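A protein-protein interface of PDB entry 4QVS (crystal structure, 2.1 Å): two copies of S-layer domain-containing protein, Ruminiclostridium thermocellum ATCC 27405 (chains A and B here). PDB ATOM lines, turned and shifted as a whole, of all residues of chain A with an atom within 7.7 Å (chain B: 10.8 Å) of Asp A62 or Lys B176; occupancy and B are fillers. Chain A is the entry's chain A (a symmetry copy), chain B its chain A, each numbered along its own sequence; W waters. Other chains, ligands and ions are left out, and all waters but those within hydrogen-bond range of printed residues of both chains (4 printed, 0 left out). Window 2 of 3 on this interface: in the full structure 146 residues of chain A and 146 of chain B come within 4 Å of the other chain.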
ATOM      1  N   HIS A  29     -10.136   8.988  -6.555  1.00  0.00           N
ATOM      2  CA  HIS A  29     -11.214   9.127  -7.532  1.00  0.00           C
ATOM      3  C   HIS A  29     -10.770  10.010  -8.668  1.00  0.00           C
ATOM      4  O   HIS A  29      -9.779  10.758  -8.556  1.00  0.00           O
ATOM      5  CB  HIS A  29     -12.519   9.636  -6.865  1.00  0.00           C
ATOM      6  CG  HIS A  29     -12.983   8.765  -5.739  1.00  0.00           C
ATOM      7  ND1 HIS A  29     -13.762   7.638  -5.932  1.00  0.00           N
ATOM      8  CD2 HIS A  29     -12.739   8.827  -4.408  1.00  0.00           C
ATOM      9  CE1 HIS A  29     -13.987   7.058  -4.768  1.00  0.00           C
ATOM     10  NE2 HIS A  29     -13.366   7.752  -3.829  1.00  0.00           N
ATOM     11  N   GLY A  30     -11.481   9.866  -9.785  1.00  0.00           N
ATOM     12  CA  GLY A  30     -11.237  10.663 -10.978  1.00  0.00           C
ATOM     13  C   GLY A  30     -11.469  12.147 -10.797  1.00  0.00           C
ATOM     14  O   GLY A  30     -11.870  12.630  -9.712  1.00  0.00           O
ATOM     15  N   ASN A  31     -11.231  12.873 -11.879  1.00  0.00           N
ATOM     16  CA  ASN A  31     -11.333  14.300 -11.860  1.00  0.00           C
ATOM     17  C   ASN A  31     -12.750  14.807 -11.811  1.00  0.00           C
ATOM     18  O   ASN A  31     -13.636  14.231 -12.445  1.00  0.00           O
ATOM     19  CB  ASN A  31     -10.637  14.876 -13.077  1.00  0.00           C
ATOM     20  CG  ASN A  31      -9.161  14.565 -13.095  1.00  0.00           C
ATOM     21  OD1 ASN A  31      -8.569  14.313 -12.036  1.00  0.00           O
ATOM     22  ND2 ASN A  31      -8.551  14.576 -14.287  1.00  0.00           N
ATOM     23  N   ALA A  59     -19.578  18.064 -12.265  1.00  0.00           N
ATOM     24  CA  ALA A  59     -19.828  16.655 -12.393  1.00  0.00           C
ATOM     25  C   ALA A  59     -18.734  15.966 -11.613  1.00  0.00           C
ATOM     26  O   ALA A  59     -17.549  16.265 -11.785  1.00  0.00           O
ATOM     27  CB  ALA A  59     -19.790  16.185 -13.867  1.00  0.00           C
ATOM     28  N   LEU A  60     -19.130  15.044 -10.744  1.00  0.00           N
ATOM     29  CA  LEU A  60     -18.184  14.265  -9.965  1.00  0.00           C
ATOM     30  C   LEU A  60     -18.084  12.933 -10.676  1.00  0.00           C
ATOM     31  O   LEU A  60     -18.982  12.562 -11.432  1.00  0.00           O
ATOM     32  CB  LEU A  60     -18.699  14.064  -8.548  1.00  0.00           C
ATOM     33  CG  LEU A  60     -18.803  15.359  -7.715  1.00  0.00           C
ATOM     34  CD1 LEU A  60     -19.558  15.102  -6.431  1.00  0.00           C
ATOM     35  CD2 LEU A  60     -17.426  15.880  -7.384  1.00  0.00           C
ATOM     36  N   PRO A  61     -17.014  12.193 -10.432  1.00  0.00           N
ATOM     37  CA  PRO A  61     -16.923  10.891 -11.169  1.00  0.00           C
ATOM     38  C   PRO A  61     -17.887   9.874 -10.580  1.00  0.00           C
ATOM     39  O   PRO A  61     -18.220   9.940  -9.372  1.00  0.00           O
ATOM     40  CB  PRO A  61     -15.463  10.462 -10.967  1.00  0.00           C
ATOM     41  CG  PRO A  61     -14.977  11.269  -9.780  1.00  0.00           C
ATOM     42  CD  PRO A  61     -15.778  12.544  -9.722  1.00  0.00           C
ATOM     43  N   ASP A  62     -18.377   8.977 -11.433  1.00  0.00           N
ATOM     44  CA  ASP A  62     -19.341   7.952 -11.050  1.00  0.00           C
ATOM     45  C   ASP A  62     -18.801   7.120  -9.905  1.00  0.00           C
ATOM     46  O   ASP A  62     -17.620   6.853  -9.864  1.00  0.00           O
ATOM     47  CB  ASP A  62     -19.600   6.965 -12.227  1.00  0.00           C
ATOM     48  CG  ASP A  62     -20.124   7.642 -13.491  1.00  0.00           C
ATOM     49  OD1 ASP A  62     -20.421   8.860 -13.481  1.00  0.00           O
ATOM     50  OD2 ASP A  62     -20.238   6.932 -14.531  1.00  0.00           O
ATOM     51  N   GLY A  63     -19.667   6.675  -9.007  1.00  0.00           N
ATOM     52  CA  GLY A  63     -19.287   5.786  -7.903  1.00  0.00           C
ATOM     53  C   GLY A  63     -18.708   6.452  -6.651  1.00  0.00           C
ATOM     54  O   GLY A  63     -18.543   5.834  -5.621  1.00  0.00           O
ATOM     55  N   ILE A  64     -18.453   7.727  -6.716  1.00  0.00           N
ATOM     56  CA  ILE A  64     -17.760   8.356  -5.615  1.00  0.00           C
ATOM     57  C   ILE A  64     -18.387   8.138  -4.230  1.00  0.00           C
ATOM     58  O   ILE A  64     -17.642   7.973  -3.277  1.00  0.00           O
ATOM     59  CB  ILE A  64     -17.407   9.818  -5.947  1.00  0.00           C
ATOM     60  CG1 ILE A  64     -16.360  10.306  -4.939  1.00  0.00           C
ATOM     61  CG2 ILE A  64     -18.655  10.706  -6.048  1.00  0.00           C
ATOM     62  CD1 ILE A  64     -15.726  11.606  -5.373  1.00  0.00           C
ATOM     63  N   ALA A  65     -19.723   8.024  -4.142  1.00  0.00           N
ATOM     64  CA  ALA A  65     -20.412   7.812  -2.849  1.00  0.00           C
ATOM     65  C   ALA A  65     -21.292   6.568  -2.675  1.00  0.00           C
ATOM     66  O   ALA A  65     -21.747   6.313  -1.557  1.00  0.00           O
ATOM     67  CB  ALA A  65     -21.235   9.044  -2.486  1.00  0.00           C
ATOM     68  N   GLY A  66     -21.498   5.771  -3.714  1.00  0.00           N
ATOM     69  CA  GLY A  66     -22.421   4.629  -3.618  1.00  0.00           C
ATOM     70  C   GLY A  66     -21.901   3.293  -3.116  1.00  0.00           C
ATOM     71  O   GLY A  66     -22.552   2.264  -3.313  1.00  0.00           O
ATOM     72  N   ASP A  89     -26.218  16.064  -5.441  1.00  0.00           N
ATOM     73  CA  ASP A  89     -27.177  14.999  -5.798  1.00  0.00           C
ATOM     74  C   ASP A  89     -26.362  13.837  -6.291  1.00  0.00           C
ATOM     75  O   ASP A  89     -25.506  13.995  -7.133  1.00  0.00           O
ATOM     76  CB  ASP A  89     -28.180  15.566  -6.785  1.00  0.00           C
ATOM     77  CG  ASP A  89     -29.126  14.545  -7.356  1.00  0.00           C
ATOM     78  OD1 ASP A  89     -29.416  13.515  -6.754  1.00  0.00           O
ATOM     79  OD2 ASP A  89     -29.693  14.875  -8.400  1.00  0.00           O
ATOM     80  N   PHE A  90     -26.551  12.706  -5.620  1.00  0.00           N
ATOM     81  CA  PHE A  90     -25.922  11.470  -5.939  1.00  0.00           C
ATOM     82  C   PHE A  90     -27.104  10.557  -6.165  1.00  0.00           C
ATOM     83  O   PHE A  90     -27.946  10.353  -5.283  1.00  0.00           O
ATOM     84  CB  PHE A  90     -25.024  10.951  -4.827  1.00  0.00           C
ATOM     85  CG  PHE A  90     -23.865  11.867  -4.516  1.00  0.00           C
ATOM     86  CD1 PHE A  90     -22.687  11.796  -5.227  1.00  0.00           C
ATOM     87  CD2 PHE A  90     -23.979  12.819  -3.514  1.00  0.00           C
ATOM     88  CE1 PHE A  90     -21.620  12.649  -4.927  1.00  0.00           C
ATOM     89  CE2 PHE A  90     -22.916  13.671  -3.203  1.00  0.00           C
ATOM     90  CZ  PHE A  90     -21.742  13.590  -3.913  1.00  0.00           C
ATOM     91  N   PHE A  91     -27.172  10.007  -7.367  1.00  0.00           N
ATOM     92  CA  PHE A  91     -28.360   9.257  -7.781  1.00  0.00           C
ATOM     93  C   PHE A  91     -28.007   8.028  -8.641  1.00  0.00           C
ATOM     94  O   PHE A  91     -26.979   7.989  -9.284  1.00  0.00           O
ATOM     95  CB  PHE A  91     -29.281  10.227  -8.555  1.00  0.00           C
ATOM     96  CG  PHE A  91     -28.635  10.870  -9.781  1.00  0.00           C
ATOM     97  CD1 PHE A  91     -27.808  11.974  -9.659  1.00  0.00           C
ATOM     98  CD2 PHE A  91     -28.893  10.377 -11.059  1.00  0.00           C
ATOM     99  CE1 PHE A  91     -27.223  12.554 -10.760  1.00  0.00           C
ATOM    100  CE2 PHE A  91     -28.303  10.947 -12.184  1.00  0.00           C
ATOM    101  CZ  PHE A  91     -27.474  12.041 -12.044  1.00  0.00           C
ATOM    102  N   ASP A  92     -28.860   7.018  -8.572  1.00  0.00           N
ATOM    103  CA  ASP A  92     -28.726   5.759  -9.315  1.00  0.00           C
ATOM    104  C   ASP A  92     -28.691   6.078 -10.796  1.00  0.00           C
ATOM    105  O   ASP A  92     -29.549   6.814 -11.276  1.00  0.00           O
ATOM    106  CB  ASP A  92     -29.952   4.870  -8.993  1.00  0.00           C
ATOM    107  CG  ASP A  92     -30.033   3.579  -9.843  1.00  0.00           C
ATOM    108  OD1 ASP A  92     -29.013   3.075 -10.305  1.00  0.00           O
ATOM    109  OD2 ASP A  92     -31.139   3.065 -10.054  1.00  0.00           O
ATOM    110  N   SER A  93     -27.689   5.572 -11.512  1.00  0.00           N
ATOM    111  CA  SER A  93     -27.640   5.781 -12.957  1.00  0.00           C
ATOM    112  C   SER A  93     -28.772   4.968 -13.678  1.00  0.00           C
ATOM    113  O   SER A  93     -29.192   5.316 -14.782  1.00  0.00           O
ATOM    114  CB  SER A  93     -26.257   5.410 -13.523  1.00  0.00           C
ATOM    115  OG  SER A  93     -26.001   4.006 -13.444  1.00  0.00           O
ATOM    116  N   GLY A  94     -29.271   3.908 -13.055  1.00  0.00           N
ATOM    117  CA  GLY A  94     -30.353   3.089 -13.643  1.00  0.00           C
ATOM    118  C   GLY A  94     -31.800   3.519 -13.424  1.00  0.00           C
ATOM    119  O   GLY A  94     -32.701   2.957 -14.012  1.00  0.00           O
ATOM    120  N   LYS A  98     -34.079   6.779  -6.923  1.00  0.00           N
ATOM    121  CA  LYS A  98     -33.140   6.230  -5.973  1.00  0.00           C
ATOM    122  C   LYS A  98     -31.988   7.232  -5.911  1.00  0.00           C
ATOM    123  O   LYS A  98     -31.139   7.294  -6.814  1.00  0.00           O
ATOM    124  CB  LYS A  98     -32.624   4.875  -6.430  1.00  0.00           C
ATOM    125  CG  LYS A  98     -33.587   3.714  -6.225  1.00  0.00           C
ATOM    126  CD  LYS A  98     -32.853   2.381  -6.419  1.00  0.00           C
ATOM    127  CE  LYS A  98     -33.756   1.172  -6.260  1.00  0.00           C
ATOM    128  NZ  LYS A  98     -34.794   1.090  -7.320  1.00  0.00           N
ATOM    129  N   TYR A  99     -31.957   8.025  -4.851  1.00  0.00           N
ATOM    130  CA  TYR A  99     -30.974   9.095  -4.789  1.00  0.00           C
ATOM    131  C   TYR A  99     -30.889   9.708  -3.405  1.00  0.00           C
ATOM    132  O   TYR A  99     -31.726   9.405  -2.553  1.00  0.00           O
ATOM    133  CB  TYR A  99     -31.385  10.223  -5.761  1.00  0.00           C
ATOM    134  CG  TYR A  99     -32.739  10.918  -5.493  1.00  0.00           C
ATOM    135  CD1 TYR A  99     -32.842  12.013  -4.608  1.00  0.00           C
ATOM    136  CD2 TYR A  99     -33.890  10.523  -6.166  1.00  0.00           C
ATOM    137  CE1 TYR A  99     -34.057  12.643  -4.382  1.00  0.00           C
ATOM    138  CE2 TYR A  99     -35.103  11.139  -5.964  1.00  0.00           C
ATOM    139  CZ  TYR A  99     -35.184  12.202  -5.072  1.00  0.00           C
ATOM    140  OH  TYR A  99     -36.389  12.802  -4.901  1.00  0.00           O
ATOM    141  N   MET A 100     -29.875  10.564  -3.216  1.00  0.00           N
ATOM    142  CA  MET A 100     -29.756  11.365  -1.995  1.00  0.00           C
ATOM    143  C   MET A 100     -29.305  12.702  -2.509  1.00  0.00           C
ATOM    144  O   MET A 100     -28.491  12.788  -3.417  1.00  0.00           O
ATOM    145  CB  MET A 100     -29.003  10.673  -0.872  1.00  0.00           C
ATOM    146  CG  MET A 100     -27.502  10.803  -0.996  1.00  0.00           C
ATOM    147  SD  MET A 100     -26.662   9.407   0.097  1.00  0.00           S
ATOM    148  CE  MET A 100     -25.038  10.305  -0.383  1.00  0.00           C
ATOM    149  N   PRO B 167     -30.144   3.162  -0.807  1.00  0.00           N
ATOM    150  CA  PRO B 167     -30.723   3.454  -2.128  1.00  0.00           C
ATOM    151  C   PRO B 167     -29.753   3.186  -3.288  1.00  0.00           C
ATOM    152  O   PRO B 167     -30.099   2.514  -4.251  1.00  0.00           O
ATOM    153  CB  PRO B 167     -31.086   4.950  -2.042  1.00  0.00           C
ATOM    154  CG  PRO B 167     -30.344   5.502  -0.869  1.00  0.00           C
ATOM    155  CD  PRO B 167     -29.699   4.377  -0.100  1.00  0.00           C
ATOM    156  N   LEU B 168     -28.551   3.743  -3.183  1.00  0.00           N
ATOM    157  CA  LEU B 168     -27.489   3.590  -4.178  1.00  0.00           C
ATOM    158  C   LEU B 168     -26.632   2.410  -3.800  1.00  0.00           C
ATOM    159  O   LEU B 168     -26.157   1.697  -4.671  1.00  0.00           O
ATOM    160  CB  LEU B 168     -26.572   4.824  -4.181  1.00  0.00           C
ATOM    161  CG  LEU B 168     -27.050   6.226  -4.604  1.00  0.00           C
ATOM    162  CD1 LEU B 168     -28.439   6.594  -4.112  1.00  0.00           C
ATOM    163  CD2 LEU B 168     -26.042   7.265  -4.132  1.00  0.00           C
ATOM    164  N   THR B 169     -26.426   2.255  -2.488  1.00  0.00           N
ATOM    165  CA  THR B 169     -25.579   1.224  -1.885  1.00  0.00           C
ATOM    166  C   THR B 169     -26.328  -0.092  -1.696  1.00  0.00           C
ATOM    167  O   THR B 169     -27.320  -0.087  -0.968  1.00  0.00           O
ATOM    168  CB  THR B 169     -25.187   1.684  -0.463  1.00  0.00           C
ATOM    169  OG1 THR B 169     -25.246   3.118  -0.384  1.00  0.00           O
ATOM    170  CG2 THR B 169     -23.822   1.125  -0.050  1.00  0.00           C
ATOM    171  N   LEU B 171     -24.465  -1.471  -5.686  1.00  0.00           N
ATOM    172  CA  LEU B 171     -24.718  -1.218  -7.130  1.00  0.00           C
ATOM    173  C   LEU B 171     -24.516   0.287  -7.369  1.00  0.00           C
ATOM    174  O   LEU B 171     -24.863   0.834  -8.421  1.00  0.00           O
ATOM    175  CB  LEU B 171     -26.061  -1.748  -7.674  1.00  0.00           C
ATOM    176  CG  LEU B 171     -26.022  -3.206  -8.150  1.00  0.00           C
ATOM    177  CD1 LEU B 171     -25.593  -4.143  -7.028  1.00  0.00           C
ATOM    178  CD2 LEU B 171     -27.357  -3.637  -8.748  1.00  0.00           C
ATOM    179  N   GLY B 172     -23.890   0.920  -6.373  1.00  0.00           N
ATOM    180  CA  GLY B 172     -23.584   2.329  -6.385  1.00  0.00           C
ATOM    181  C   GLY B 172     -22.347   2.610  -7.207  1.00  0.00           C
ATOM    182  O   GLY B 172     -22.092   3.763  -7.517  1.00  0.00           O
ATOM    183  N   GLU B 173     -21.569   1.573  -7.534  1.00  0.00           N
ATOM    184  CA  GLU B 173     -20.408   1.689  -8.446  1.00  0.00           C
ATOM    185  C   GLU B 173     -20.642   2.665  -9.649  1.00  0.00           C
ATOM    186  O   GLU B 173     -19.794   3.527  -9.932  1.00  0.00           O
ATOM    187  CB  GLU B 173     -19.982   0.291  -8.935  1.00  0.00           C
ATOM    188  CG  GLU B 173     -21.153  -0.628  -9.290  1.00  0.00           C
ATOM    189  CD  GLU B 173     -20.751  -1.871 -10.063  1.00  0.00           C
ATOM    190  OE1 GLU B 173     -21.607  -2.768 -10.193  1.00  0.00           O
ATOM    191  OE2 GLU B 173     -19.602  -1.957 -10.551  1.00  0.00           O
ATOM    192  N   THR B 174     -21.787   2.556 -10.327  1.00  0.00           N
ATOM    193  CA  THR B 174     -22.122   3.468 -11.436  1.00  0.00           C
ATOM    194  C   THR B 174     -22.986   4.703 -10.997  1.00  0.00           C
ATOM    195  O   THR B 174     -23.619   5.366 -11.796  1.00  0.00           O
ATOM    196  CB  THR B 174     -22.909   2.698 -12.506  1.00  0.00           C
ATOM    197  OG1 THR B 174     -24.178   2.374 -11.955  1.00  0.00           O
ATOM    198  CG2 THR B 174     -22.179   1.420 -12.894  1.00  0.00           C
ATOM    199  N   SER B 175     -23.024   5.050  -9.726  1.00  0.00           N
ATOM    200  CA  SER B 175     -23.845   6.217  -9.333  1.00  0.00           C
ATOM    201  C   SER B 175     -23.284   7.545  -9.882  1.00  0.00           C
ATOM    202  O   SER B 175     -22.079   7.700 -10.025  1.00  0.00           O
ATOM    203  CB  SER B 175     -23.962   6.264  -7.827  1.00  0.00           C
ATOM    204  OG  SER B 175     -22.675   6.311  -7.264  1.00  0.00           O
ATOM    205  N   LYS B 176     -24.170   8.478 -10.207  1.00  0.00           N
ATOM    206  CA  LYS B 176     -23.817   9.775 -10.757  1.00  0.00           C
ATOM    207  C   LYS B 176     -23.839  10.836  -9.633  1.00  0.00           C
ATOM    208  O   LYS B 176     -24.585  10.701  -8.676  1.00  0.00           O
ATOM    209  CB  LYS B 176     -24.835  10.177 -11.809  1.00  0.00           C
ATOM    210  CG  LYS B 176     -24.950   9.279 -13.045  1.00  0.00           C
ATOM    211  CD  LYS B 176     -23.663   9.259 -13.839  1.00  0.00           C
ATOM    212  CE  LYS B 176     -23.853   8.721 -15.251  1.00  0.00           C
ATOM    213  NZ  LYS B 176     -22.536   8.504 -15.932  1.00  0.00           N
ATOM    214  N   GLY B 177     -23.047  11.881  -9.777  1.00  0.00           N
ATOM    215  CA  GLY B 177     -22.985  12.927  -8.769  1.00  0.00           C
ATOM    216  C   GLY B 177     -22.802  14.283  -9.389  1.00  0.00           C
ATOM    217  O   GLY B 177     -22.005  14.438 -10.329  1.00  0.00           O
ATOM    218  N   TYR B 178     -23.583  15.246  -8.887  1.00  0.00           N
ATOM    219  CA  TYR B 178     -23.429  16.646  -9.232  1.00  0.00           C
ATOM    220  C   TYR B 178     -23.272  17.520  -7.999  1.00  0.00           C
ATOM    221  O   TYR B 178     -23.724  17.179  -6.922  1.00  0.00           O
ATOM    222  CB  TYR B 178     -24.680  17.177  -9.882  1.00  0.00           C
ATOM    223  CG  TYR B 178     -25.112  16.525 -11.165  1.00  0.00           C
ATOM    224  CD1 TYR B 178     -24.223  16.352 -12.203  1.00  0.00           C
ATOM    225  CD2 TYR B 178     -26.434  16.157 -11.346  1.00  0.00           C
ATOM    226  CE1 TYR B 178     -24.617  15.786 -13.422  1.00  0.00           C
ATOM    227  CE2 TYR B 178     -26.862  15.615 -12.568  1.00  0.00           C
ATOM    228  CZ  TYR B 178     -25.937  15.398 -13.570  1.00  0.00           C
ATOM    229  OH  TYR B 178     -26.336  14.858 -14.722  1.00  0.00           O
ATOM    230  N   ILE B 179     -22.667  18.670  -8.200  1.00  0.00           N
ATOM    231  CA  ILE B 179     -22.699  19.719  -7.213  1.00  0.00           C
ATOM    232  C   ILE B 179     -23.410  20.820  -7.954  1.00  0.00           C
ATOM    233  O   ILE B 179     -22.933  21.267  -8.984  1.00  0.00           O
ATOM    234  CB  ILE B 179     -21.303  20.237  -6.797  1.00  0.00           C
ATOM    235  CG1 ILE B 179     -20.516  19.153  -6.090  1.00  0.00           C
ATOM    236  CG2 ILE B 179     -21.430  21.422  -5.866  1.00  0.00           C
ATOM    237  CD1 ILE B 179     -19.074  19.523  -5.776  1.00  0.00           C
ATOM    238  N   GLY B 180     -24.531  21.296  -7.421  1.00  0.00           N
ATOM    239  CA  GLY B 180     -25.207  22.437  -8.018  1.00  0.00           C
ATOM    240  C   GLY B 180     -26.280  22.174  -9.078  1.00  0.00           C
ATOM    241  O   GLY B 180     -26.859  23.116  -9.620  1.00  0.00           O
ATOM    242  N   LYS B 181     -26.546  20.903  -9.334  1.00  0.00           N
ATOM    243  CA  LYS B 181     -27.517  20.483 -10.309  1.00  0.00           C
ATOM    244  C   LYS B 181     -28.141  19.267  -9.681  1.00  0.00           C
ATOM    245  O   LYS B 181     -27.515  18.580  -8.864  1.00  0.00           O
ATOM    246  CB  LYS B 181     -26.801  20.116 -11.616  1.00  0.00           C
ATOM    247  CG  LYS B 181     -27.644  19.524 -12.754  1.00  0.00           C
ATOM    248  CD  LYS B 181     -26.751  19.258 -13.954  1.00  0.00           C
ATOM    249  CE  LYS B 181     -27.517  18.489 -15.050  1.00  0.00           C
ATOM    250  NZ  LYS B 181     -26.671  18.403 -16.245  1.00  0.00           N
ATOM    251  N   SER B 182     -29.411  19.078  -9.988  1.00  0.00           N
ATOM    252  CA  SER B 182     -30.106  17.870  -9.656  1.00  0.00           C
ATOM    253  C   SER B 182     -30.453  17.100 -10.964  1.00  0.00           C
ATOM    254  O   SER B 182     -30.666  17.709 -12.004  1.00  0.00           O
ATOM    255  CB  SER B 182     -31.419  18.190  -9.009  1.00  0.00           C
ATOM    256  OG  SER B 182     -32.165  16.995  -8.836  1.00  0.00           O
ATOM    257  N   HIS B 183     -30.536  15.791 -10.874  1.00  0.00           N
ATOM    258  CA  HIS B 183     -31.072  14.975 -11.987  1.00  0.00           C
ATOM    259  C   HIS B 183     -32.594  15.115 -11.977  1.00  0.00           C
ATOM    260  O   HIS B 183     -33.189  15.648 -11.013  1.00  0.00           O
ATOM    261  CB  HIS B 183     -30.718  13.497 -11.806  1.00  0.00           C
ATOM    262  CG  HIS B 183     -31.550  12.786 -10.787  1.00  0.00           C
ATOM    263  ND1 HIS B 183     -31.411  13.002  -9.429  1.00  0.00           N
ATOM    264  CD2 HIS B 183     -32.479  11.803 -10.921  1.00  0.00           C
ATOM    265  CE1 HIS B 183     -32.252  12.222  -8.776  1.00  0.00           C
ATOM    266  NE2 HIS B 183     -32.923  11.491  -9.658  1.00  0.00           N
ATOM    267  N   GLN B 184     -33.235  14.593 -13.023  1.00  0.00           N
ATOM    268  CA  GLN B 184     -34.677  14.661 -13.148  1.00  0.00           C
ATOM    269  C   GLN B 184     -35.280  13.548 -12.344  1.00  0.00           C
ATOM    270  O   GLN B 184     -35.020  12.370 -12.644  1.00  0.00           O
ATOM    271  CB  GLN B 184     -35.098  14.465 -14.624  1.00  0.00           C
ATOM    272  CG  GLN B 184     -36.556  14.815 -14.838  1.00  0.00           C
ATOM    273  CD  GLN B 184     -37.008  14.646 -16.275  1.00  0.00           C
ATOM    274  OE1 GLN B 184     -36.469  13.841 -17.023  1.00  0.00           O
ATOM    275  NE2 GLN B 184     -38.027  15.392 -16.652  1.00  0.00           N
ATOM    276  N   PHE B 204     -14.608  20.274  -1.320  1.00  0.00           N
ATOM    277  CA  PHE B 204     -15.671  19.305  -1.271  1.00  0.00           C
ATOM    278  C   PHE B 204     -15.029  17.979  -0.888  1.00  0.00           C
ATOM    279  O   PHE B 204     -14.118  17.491  -1.557  1.00  0.00           O
ATOM    280  CB  PHE B 204     -16.383  19.212  -2.604  1.00  0.00           C
ATOM    281  CG  PHE B 204     -17.681  18.497  -2.533  1.00  0.00           C
ATOM    282  CD1 PHE B 204     -17.739  17.134  -2.690  1.00  0.00           C
ATOM    283  CD2 PHE B 204     -18.858  19.202  -2.346  1.00  0.00           C
ATOM    284  CE1 PHE B 204     -18.955  16.475  -2.650  1.00  0.00           C
ATOM    285  CE2 PHE B 204     -20.076  18.560  -2.321  1.00  0.00           C
ATOM    286  CZ  PHE B 204     -20.127  17.187  -2.467  1.00  0.00           C
ATOM    287  N   ILE B 206     -15.483  13.913   0.946  1.00  0.00           N
ATOM    288  CA  ILE B 206     -16.309  12.745   1.126  1.00  0.00           C
ATOM    289  C   ILE B 206     -15.533  11.737   1.926  1.00  0.00           C
ATOM    290  O   ILE B 206     -14.352  11.517   1.664  1.00  0.00           O
ATOM    291  CB  ILE B 206     -16.656  12.139  -0.245  1.00  0.00           C
ATOM    292  CG1 ILE B 206     -17.479  13.152  -1.043  1.00  0.00           C
ATOM    293  CG2 ILE B 206     -17.415  10.835  -0.075  1.00  0.00           C
ATOM    294  CD1 ILE B 206     -17.671  12.782  -2.490  1.00  0.00           C
HETATM  295  O   HOH W   1     -20.851   9.801  -8.291  1.00  0.00           O
HETATM  296  O   HOH W   2     -22.831   5.457 -14.341  1.00  0.00           O
HETATM  297  O   HOH W   3     -32.355   8.177  -9.315  1.00  0.00           O
HETATM  298  O   HOH W   4     -21.086  11.356 -12.047  1.00  0.00           O
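The backbone carbonyl oxygen of Glu B173 lies close to the backbone NH of Gly A63.
OG of Ser A93 is in hydrogen-bond range of OG1 of Thr B174 (2.9 Å).
O of Ser B175 lies within hydrogen-bond range of N of Gly A63 (2.8 Å).
OD2 of Asp A62 is in salt-bridge range of NZ of Lys B176.
The backbone NH of Phe A91 sits at hydrogen-bond distance from the backbone carbonyl oxygen of Lys B176.
N of Leu A60 lies within hydrogen-bond range of O of Gly B177 (3.0 Å).
The backbone NH (N) of Tyr B178 lies within hydrogen-bond range of the backbone carbonyl oxygen (O) of Asp A89.
The side-chain carboxylate (OD2) of Asp A89 sits close to the side-chain hydroxyl (OG) of Ser B182 (3.3 Å).
A ring nitrogen (ND1) of His B183 sits at hydrogen-bond distance from the side-chain carboxylate of Asp A89 (2.7 Å).
The backbone carbonyl oxygen (O) of Gly B172 sits at hydrogen-bond distance from the side-chain hydroxyl (OG) of Ser B175 (2.6 Å).
The backbone NH (N) of Met A100 sits at hydrogen-bond distance from the backbone carbonyl oxygen (O) of Phe A90 (2.8 Å).
The backbone carbonyl oxygen of Lys A98 is in hydrogen-bond range of the backbone NH of Asp A92 (2.9 Å).
Asp A62 touches Glu B173 (C to O, 3.7 Å).
CA of Gly A63 touches O of Gly B172, 3.5 Å away.
Ile A64 touches Ile B206.
Gly B172 touches Gly A66.
Asp A89 touches Lys B176 (O to O, 3.8 Å).
O of Asp A89 touches CA of Gly B177 (3.2 Å).
O of Phe A90 touches CD2 of Leu B168, 3.8 Å away.
CG of Phe A91 touches ND1 of His B183, at 3.5 Å.
Lys A98 touches Pro B167 (CD to O, 3.5 Å).
Leu B168 touches Lys A98.
Asp A62 touches just these residues of chain B: Glu B173 (3.7 Å), Ser B175 (2.9 Å) and Lys B176 (3.1 Å).
Of chain A, only Asp A62 (3.1 Å), Asp A89 (3.8 Å), Phe A90 (3.1 Å) and Phe A91 (3.0 Å) come within 4 Å of Lys B176.
Pro A61 touches none of the printed residues of chain B.
Gly A63 touches just these residues of chain B: Gly B172, Glu B173 and Ser B175.
Of the printed residues of chain B, Phe A91 touches Ser B175 (3.6 Å), Lys B176 (3.0 Å), Tyr B178 (3.6 Å) and His B183 (3.5 Å).
Printed residues of chain A within 4 Å of His B183: Asp A89 (2.7 Å), Phe A91 (3.5 Å) and Tyr A99 (3.5 Å).
Printed residues of chain B within 4 Å of Ala A59: Gly B177 (3.7 Å).
Of the printed residues of chain A, Ser B175 touches Asp A62, Gly A63, Gly A66 and Phe A91.
Printed residues of chain B within 4 Å of Leu A60: Gly B177.
His A29 touches none of the printed residues of chain B.
The nearest residue of chain B that does not touch Asp A62 is Thr B174 (4.3 Å).
Of the 20 printed residues of chain A, 12 touch a printed residue of chain B.
Printed residues of chain A that touch a printed residue of chain B: Ala A59, Leu A60, Asp A62, Gly A63, Ile A64, Gly A66, Asp A89, Phe A90, Phe A91, Ser A93, Lys A98 and Tyr A99.
Hydrophobic or aromatic side chains of chain A that line the printed part of chain B: Leu A60, Ile A64, Phe A90, Phe A91 and Tyr A99.
Along chain A the printed residues that touch a printed residue of chain B span positions 59 to 99.
Hydrophobic or aromatic side chains of chain B that line the printed part of chain A: Leu B168, Tyr B178, His B183 and Ile B206.
Among the printed residues, 31 pairs touch across the chains.
No position is printed for both chains.
Water W2 lies within hydrogen-bond range of O of Thr B174 (2.7 Å), OD2 of Asp A62 (3.0 Å) and NZ of Lys B176 (3.5 Å).
Water W1 lies within hydrogen-bond range of the backbone carbonyl oxygen of Pro A61 (2.8 Å), the backbone carbonyl oxygen of Ser B175 (3.0 Å), the backbone NH of Gly B177 (3.4 Å) and the backbone NH of Gly A63 (3.4 Å).
Water W3 lies within hydrogen-bond range of the backbone carbonyl oxygen (O) of Lys A98 (2.9 Å) and a ring nitrogen (NE2) of His B183 (3.4 Å).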
